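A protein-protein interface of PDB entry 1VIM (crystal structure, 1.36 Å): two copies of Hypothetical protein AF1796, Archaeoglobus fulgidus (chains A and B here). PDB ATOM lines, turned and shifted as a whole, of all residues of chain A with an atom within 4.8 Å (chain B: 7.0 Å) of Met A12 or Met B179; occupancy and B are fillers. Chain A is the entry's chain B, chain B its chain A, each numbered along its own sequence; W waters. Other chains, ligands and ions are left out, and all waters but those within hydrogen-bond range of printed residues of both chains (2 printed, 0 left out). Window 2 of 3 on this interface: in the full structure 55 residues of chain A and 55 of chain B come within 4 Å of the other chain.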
ATOM      1  N   HIS A  11      31.237   7.507 -10.361  1.00  0.00           N
ATOM      2  CA  HIS A  11      30.266   6.553  -9.751  1.00  0.00           C
ATOM      3  C   HIS A  11      28.846   7.029 -10.033  1.00  0.00           C
ATOM      4  O   HIS A  11      28.069   7.338  -9.120  1.00  0.00           O
ATOM      5  CB  HIS A  11      30.529   6.411  -8.248  1.00  0.00           C
ATOM      6  CG  HIS A  11      31.898   5.899  -7.929  1.00  0.00           C
ATOM      7  ND1 HIS A  11      32.322   4.640  -8.301  1.00  0.00           N
ATOM      8  CD2 HIS A  11      32.945   6.476  -7.295  1.00  0.00           C
ATOM      9  CE1 HIS A  11      33.568   4.462  -7.899  1.00  0.00           C
ATOM     10  NE2 HIS A  11      33.970   5.562  -7.290  1.00  0.00           N
ATOM     11  N   MET A  12      28.520   7.073 -11.321  1.00  0.00           N
ATOM     12  CA  MET A  12      27.248   7.586 -11.784  1.00  0.00           C
ATOM     13  C   MET A  12      26.038   6.858 -11.205  1.00  0.00           C
ATOM     14  O   MET A  12      25.105   7.515 -10.792  1.00  0.00           O
ATOM     15  CB  MET A  12      27.189   7.672 -13.326  1.00  0.00           C
ATOM     16  CG  MET A  12      27.364   6.348 -14.104  1.00  0.00           C
ATOM     17  SD  MET A  12      28.932   5.435 -13.932  1.00  0.00           S
ATOM     18  CE  MET A  12      28.488   4.227 -12.637  1.00  0.00           C
ATOM     19  N   SER A  13      26.069   5.523 -11.172  1.00  0.00           N
ATOM     20  CA  SER A  13      24.936   4.749 -10.662  1.00  0.00           C
ATOM     21  C   SER A  13      24.703   5.001  -9.172  1.00  0.00           C
ATOM     22  O   SER A  13      23.570   5.092  -8.742  1.00  0.00           O
ATOM     23  CB  SER A  13      25.088   3.254 -10.948  1.00  0.00           C
ATOM     24  OG  SER A  13      24.925   3.022 -12.343  1.00  0.00           O
ATOM     25  N   LEU A  14      25.783   5.150  -8.409  1.00  0.00           N
ATOM     26  CA  LEU A  14      25.662   5.536  -7.007  1.00  0.00           C
ATOM     27  C   LEU A  14      24.878   6.834  -6.865  1.00  0.00           C
ATOM     28  O   LEU A  14      23.961   6.929  -6.069  1.00  0.00           O
ATOM     29  CB  LEU A  14      27.043   5.715  -6.371  1.00  0.00           C
ATOM     30  CG  LEU A  14      26.952   5.689  -4.837  1.00  0.00           C
ATOM     31  CD1 LEU A  14      28.183   5.079  -4.264  1.00  0.00           C
ATOM     32  CD2 LEU A  14      26.665   7.057  -4.216  1.00  0.00           C
ATOM     33  N   LEU A  15      25.272   7.853  -7.623  1.00  0.00           N
ATOM     34  CA  LEU A  15      24.634   9.155  -7.542  1.00  0.00           C
ATOM     35  C   LEU A  15      23.222   9.168  -8.124  1.00  0.00           C
ATOM     36  O   LEU A  15      22.344   9.825  -7.561  1.00  0.00           O
ATOM     37  CB  LEU A  15      25.509  10.212  -8.239  1.00  0.00           C
ATOM     38  CG  LEU A  15      26.927  10.389  -7.668  1.00  0.00           C
ATOM     39  CD1 LEU A  15      27.688  11.392  -8.542  1.00  0.00           C
ATOM     40  CD2 LEU A  15      26.985  10.803  -6.194  1.00  0.00           C
ATOM     41  N   ARG A  16      22.995   8.408  -9.192  1.00  0.00           N
ATOM     42  CA  ARG A  16      21.643   8.265  -9.771  1.00  0.00           C
ATOM     43  C   ARG A  16      20.685   7.576  -8.793  1.00  0.00           C
ATOM     44  O   ARG A  16      19.500   7.933  -8.709  1.00  0.00           O
ATOM     45  CB  ARG A  16      21.669   7.485 -11.092  1.00  0.00           C
ATOM     46  CG  ARG A  16      20.323   7.426 -11.824  1.00  0.00           C
ATOM     47  CD  ARG A  16      19.756   8.772 -12.262  1.00  0.00           C
ATOM     48  NE  ARG A  16      18.298   8.735 -12.345  1.00  0.00           N
ATOM     49  CZ  ARG A  16      17.504   9.785 -12.165  1.00  0.00           C
ATOM     50  NH1 ARG A  16      18.018  10.980 -11.890  1.00  0.00           N
ATOM     51  NH2 ARG A  16      16.188   9.638 -12.259  1.00  0.00           N
ATOM     52  N   GLN A 154      17.197  -1.933 -11.799  1.00  0.00           N
ATOM     53  CA  GLN A 154      18.636  -1.987 -11.903  1.00  0.00           C
ATOM     54  C   GLN A 154      19.326  -1.226 -10.763  1.00  0.00           C
ATOM     55  O   GLN A 154      20.367  -1.656 -10.285  1.00  0.00           O
ATOM     56  CB  GLN A 154      19.077  -1.429 -13.260  1.00  0.00           C
ATOM     57  CG  GLN A 154      20.571  -1.425 -13.489  1.00  0.00           C
ATOM     58  CD  GLN A 154      21.189  -2.815 -13.487  1.00  0.00           C
ATOM     59  OE1 GLN A 154      20.631  -3.757 -14.058  1.00  0.00           O
ATOM     60  NE2 GLN A 154      22.342  -2.946 -12.845  1.00  0.00           N
ATOM     61  N   LEU B  34      33.894  10.367  -3.383  1.00  0.00           N
ATOM     62  CA  LEU B  34      33.826   9.332  -4.412  1.00  0.00           C
ATOM     63  C   LEU B  34      35.098   8.487  -4.458  1.00  0.00           C
ATOM     64  O   LEU B  34      35.049   7.316  -4.806  1.00  0.00           O
ATOM     65  CB  LEU B  34      33.536   9.952  -5.785  1.00  0.00           C
ATOM     66  CG  LEU B  34      32.195  10.692  -5.858  1.00  0.00           C
ATOM     67  CD1 LEU B  34      32.044  11.461  -7.170  1.00  0.00           C
ATOM     68  CD2 LEU B  34      31.061   9.697  -5.697  1.00  0.00           C
ATOM     69  N   LEU B 173      25.678   2.070  -2.839  1.00  0.00           N
ATOM     70  CA  LEU B 173      26.896   1.341  -3.118  1.00  0.00           C
ATOM     71  C   LEU B 173      26.562   0.035  -3.857  1.00  0.00           C
ATOM     72  O   LEU B 173      27.264  -0.342  -4.804  1.00  0.00           O
ATOM     73  CB  LEU B 173      27.654   1.087  -1.803  1.00  0.00           C
ATOM     74  CG  LEU B 173      29.025   0.461  -1.942  1.00  0.00           C
ATOM     75  CD1 LEU B 173      29.977   1.530  -2.423  1.00  0.00           C
ATOM     76  CD2 LEU B 173      29.452   0.002  -0.560  1.00  0.00           C
ATOM     77  N   VAL B 174      25.501  -0.649  -3.437  1.00  0.00           N
ATOM     78  CA  VAL B 174      25.048  -1.858  -4.135  1.00  0.00           C
ATOM     79  C   VAL B 174      24.721  -1.538  -5.593  1.00  0.00           C
ATOM     80  O   VAL B 174      25.114  -2.269  -6.485  1.00  0.00           O
ATOM     81  CB  VAL B 174      23.829  -2.497  -3.415  1.00  0.00           C
ATOM     82  CG1 VAL B 174      23.136  -3.511  -4.307  1.00  0.00           C
ATOM     83  CG2 VAL B 174      24.293  -3.181  -2.146  1.00  0.00           C
ATOM     84  N   ALA B 175      23.994  -0.447  -5.840  1.00  0.00           N
ATOM     85  CA  ALA B 175      23.670  -0.047  -7.205  1.00  0.00           C
ATOM     86  C   ALA B 175      24.955   0.124  -8.021  1.00  0.00           C
ATOM     87  O   ALA B 175      25.020  -0.272  -9.193  1.00  0.00           O
ATOM     88  CB  ALA B 175      22.875   1.229  -7.171  1.00  0.00           C
ATOM     89  N   GLU B 176      25.962   0.744  -7.424  1.00  0.00           N
ATOM     90  CA  GLU B 176      27.230   0.996  -8.109  1.00  0.00           C
ATOM     91  C   GLU B 176      27.964  -0.300  -8.417  1.00  0.00           C
ATOM     92  O   GLU B 176      28.460  -0.498  -9.538  1.00  0.00           O
ATOM     93  CB  GLU B 176      28.088   1.915  -7.248  1.00  0.00           C
ATOM     94  CG  GLU B 176      29.452   2.235  -7.842  1.00  0.00           C
ATOM     95  CD  GLU B 176      29.388   3.057  -9.120  1.00  0.00           C
ATOM     96  OE1 GLU B 176      28.351   3.706  -9.397  1.00  0.00           O
ATOM     97  OE2 GLU B 176      30.416   3.048  -9.843  1.00  0.00           O
ATOM     98  N   ILE B 177      28.027  -1.203  -7.441  1.00  0.00           N
ATOM     99  CA  ILE B 177      28.651  -2.506  -7.671  1.00  0.00           C
ATOM    100  C   ILE B 177      27.907  -3.290  -8.748  1.00  0.00           C
ATOM    101  O   ILE B 177      28.539  -3.929  -9.599  1.00  0.00           O
ATOM    102  CB  ILE B 177      28.762  -3.305  -6.346  1.00  0.00           C
ATOM    103  CG1 ILE B 177      29.720  -2.594  -5.377  1.00  0.00           C
ATOM    104  CG2 ILE B 177      29.261  -4.725  -6.633  1.00  0.00           C
ATOM    105  CD1 ILE B 177      29.655  -3.073  -3.921  1.00  0.00           C
ATOM    106  N   MET B 178      26.585  -3.218  -8.762  1.00  0.00           N
ATOM    107  CA  MET B 178      25.844  -3.924  -9.815  1.00  0.00           C
ATOM    108  C   MET B 178      26.235  -3.419 -11.189  1.00  0.00           C
ATOM    109  O   MET B 178      26.462  -4.217 -12.098  1.00  0.00           O
ATOM    110  CB  MET B 178      24.349  -3.759  -9.637  1.00  0.00           C
ATOM    111  CG  MET B 178      23.793  -4.539  -8.455  1.00  0.00           C
ATOM    112  SD  MET B 178      22.096  -4.101  -8.112  1.00  0.00           S
ATOM    113  CE  MET B 178      21.235  -4.844  -9.580  1.00  0.00           C
ATOM    114  N   MET B 179      26.310  -2.101 -11.331  1.00  0.00           N
ATOM    115  CA  MET B 179      26.739  -1.490 -12.590  1.00  0.00           C
ATOM    116  C   MET B 179      28.129  -1.986 -12.986  1.00  0.00           C
ATOM    117  O   MET B 179      28.331  -2.413 -14.143  1.00  0.00           O
ATOM    118  CB  MET B 179      26.670   0.043 -12.515  1.00  0.00           C
ATOM    119  CG  MET B 179      27.113   0.769 -13.797  1.00  0.00           C
ATOM    120  SD  MET B 179      28.883   1.080 -13.806  1.00  0.00           S
ATOM    121  CE  MET B 179      29.077   1.928 -15.373  1.00  0.00           C
ATOM    122  N   GLN B 180      29.082  -1.962 -12.057  1.00  0.00           N
ATOM    123  CA  GLN B 180      30.468  -2.352 -12.350  1.00  0.00           C
ATOM    124  C   GLN B 180      30.593  -3.802 -12.767  1.00  0.00           C
ATOM    125  O   GLN B 180      31.419  -4.137 -13.631  1.00  0.00           O
ATOM    126  CB  GLN B 180      31.387  -2.080 -11.159  1.00  0.00           C
ATOM    127  CG  GLN B 180      31.582  -0.610 -10.869  1.00  0.00           C
ATOM    128  CD  GLN B 180      32.607  -0.344  -9.793  1.00  0.00           C
ATOM    129  OE1 GLN B 180      33.287  -1.259  -9.322  1.00  0.00           O
ATOM    130  NE2 GLN B 180      32.744   0.914  -9.417  1.00  0.00           N
ATOM    131  N   LYS B 181      29.757  -4.654 -12.191  1.00  0.00           N
ATOM    132  CA  LYS B 181      29.866  -6.092 -12.387  1.00  0.00           C
ATOM    133  C   LYS B 181      28.879  -6.592 -13.442  1.00  0.00           C
ATOM    134  O   LYS B 181      28.799  -7.800 -13.711  1.00  0.00           O
ATOM    135  CB  LYS B 181      29.634  -6.801 -11.049  1.00  0.00           C
ATOM    136  CG  LYS B 181      30.784  -6.657 -10.070  1.00  0.00           C
ATOM    137  CD  LYS B 181      30.441  -7.339  -8.750  1.00  0.00           C
ATOM    138  CE  LYS B 181      30.893  -8.804  -8.723  1.00  0.00           C
ATOM    139  NZ  LYS B 181      30.299  -9.586  -7.590  1.00  0.00           N
ATOM    140  N   HIS B 182      28.146  -5.654 -14.040  1.00  0.00           N
ATOM    141  CA  HIS B 182      27.103  -5.935 -15.033  1.00  0.00           C
ATOM    142  C   HIS B 182      26.083  -6.948 -14.526  1.00  0.00           C
ATOM    143  O   HIS B 182      25.696  -7.881 -15.222  1.00  0.00           O
ATOM    144  CB  HIS B 182      27.732  -6.375 -16.363  1.00  0.00           C
ATOM    145  CG  HIS B 182      28.784  -5.431 -16.855  1.00  0.00           C
ATOM    146  ND1 HIS B 182      30.130  -5.654 -16.664  1.00  0.00           N
ATOM    147  CD2 HIS B 182      28.687  -4.240 -17.492  1.00  0.00           C
ATOM    148  CE1 HIS B 182      30.819  -4.653 -17.183  1.00  0.00           C
ATOM    149  NE2 HIS B 182      29.967  -3.781 -17.693  1.00  0.00           N
ATOM    150  N   LEU B 183      25.672  -6.751 -13.273  1.00  0.00           N
ATOM    151  CA  LEU B 183      24.660  -7.581 -12.655  1.00  0.00           C
ATOM    152  C   LEU B 183      23.315  -6.899 -12.768  1.00  0.00           C
ATOM    153  O   LEU B 183      23.238  -5.673 -12.731  1.00  0.00           O
ATOM    154  CB  LEU B 183      24.991  -7.820 -11.180  1.00  0.00           C
ATOM    155  CG  LEU B 183      26.249  -8.647 -10.918  1.00  0.00           C
ATOM    156  CD1 LEU B 183      26.612  -8.558  -9.426  1.00  0.00           C
ATOM    157  CD2 LEU B 183      26.008 -10.084 -11.333  1.00  0.00           C
HETATM  158  O   HOH W   1      22.844  -0.578 -10.823  1.00  0.00           O
HETATM  159  O   HOH W   2      36.655   6.053  -7.013  1.00  0.00           O
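No position is printed for both chains.
ND1 of His A11 touches NE2 of Gln B180, 3.9 Å away.
Met A12 touches Glu B176 (CE to OE1, 3.3 Å).
Met A12 touches Met B179 (CE to SD, 3.4 Å).
CB of Ser A13 touches O of Ala B175, at 3.9 Å.
Ser A13 touches Met B179.
Of the 7 printed residues of chain A, 5 touch a printed residue of chain B.
Hydrophobic or aromatic side chains of chain A within 4 Å of the printed part of chain B: His A11, Met A12 and Leu A14.
Among the printed residues, no Asp or Glu carboxylate lies within 4 Å of a Lys or Arg side-chain nitrogen of the other chain.
OE2 of Glu B176 lies within hydrogen-bond range of ND1 of His A11 (2.9 Å).
OE1 of Glu B176 lies within hydrogen-bond range of N of Ser A13, 3.4 Å away.
The backbone carbonyl oxygen (O) of Gln A154 sits close to the side-chain sulfur (SD) of Met B178, 3.7 Å away.
O of Leu B183 lies within hydrogen-bond range of NE2 of Gln A154 (2.9 Å).
A ring nitrogen (NE2) of His A11 sits at hydrogen-bond distance from the backbone carbonyl oxygen of Leu B34 (3.2 Å).
The backbone NH (N) of Leu A14 sits at hydrogen-bond distance from the side-chain carboxylate (OE1) of Glu B176.
Printed residues of chain B within 4 Å of Met A12: Glu B176 (3.3 Å) and Met B179 (3.4 Å).
Of the printed residues of chain B, Ser A13 touches Ala B175 (3.9 Å), Glu B176 (3.4 Å) and Met B179 (3.5 Å).
Printed residues of chain B within 4 Å of Gln A154: Met B178 and Leu B183.
Printed residues of chain A within 4 Å of Leu B34: His A11 (3.2 Å).
Val B174 touches none of the printed residues of chain A.
Printed residues of chain A within 4 Å of Glu B176: His A11 (2.9 Å), Met A12 (3.3 Å), Ser A13 (3.4 Å) and Leu A14 (3.1 Å).
Of the printed residues of chain A, Met B178 touches Gln A154.
Printed residues of chain A within 4 Å of Met B179: Met A12 (3.4 Å) and Ser A13 (3.5 Å).
The nearest printed residue of chain B that does not touch Met A12 is Gln B180 (6.0 Å).
The nearest printed residue of chain A that does not touch Met B179 is Gln A154 (4.3 Å).
The side-chain carboxylate (OE2) of Glu B176 sits at hydrogen-bond distance from the side-chain amide nitrogen (NE2) of Gln B180, at 3.2 Å.
The backbone carbonyl oxygen of Met B178 sits at hydrogen-bond distance from the backbone NH of Leu B183 (2.9 Å).
Water W1 lies within hydrogen-bond range of O of Ala B175 and O of Gln A154.
Water W2 lies within hydrogen-bond range of NE2 of His A11 (2.7 Å) and O of Leu B34 (3.0 Å).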
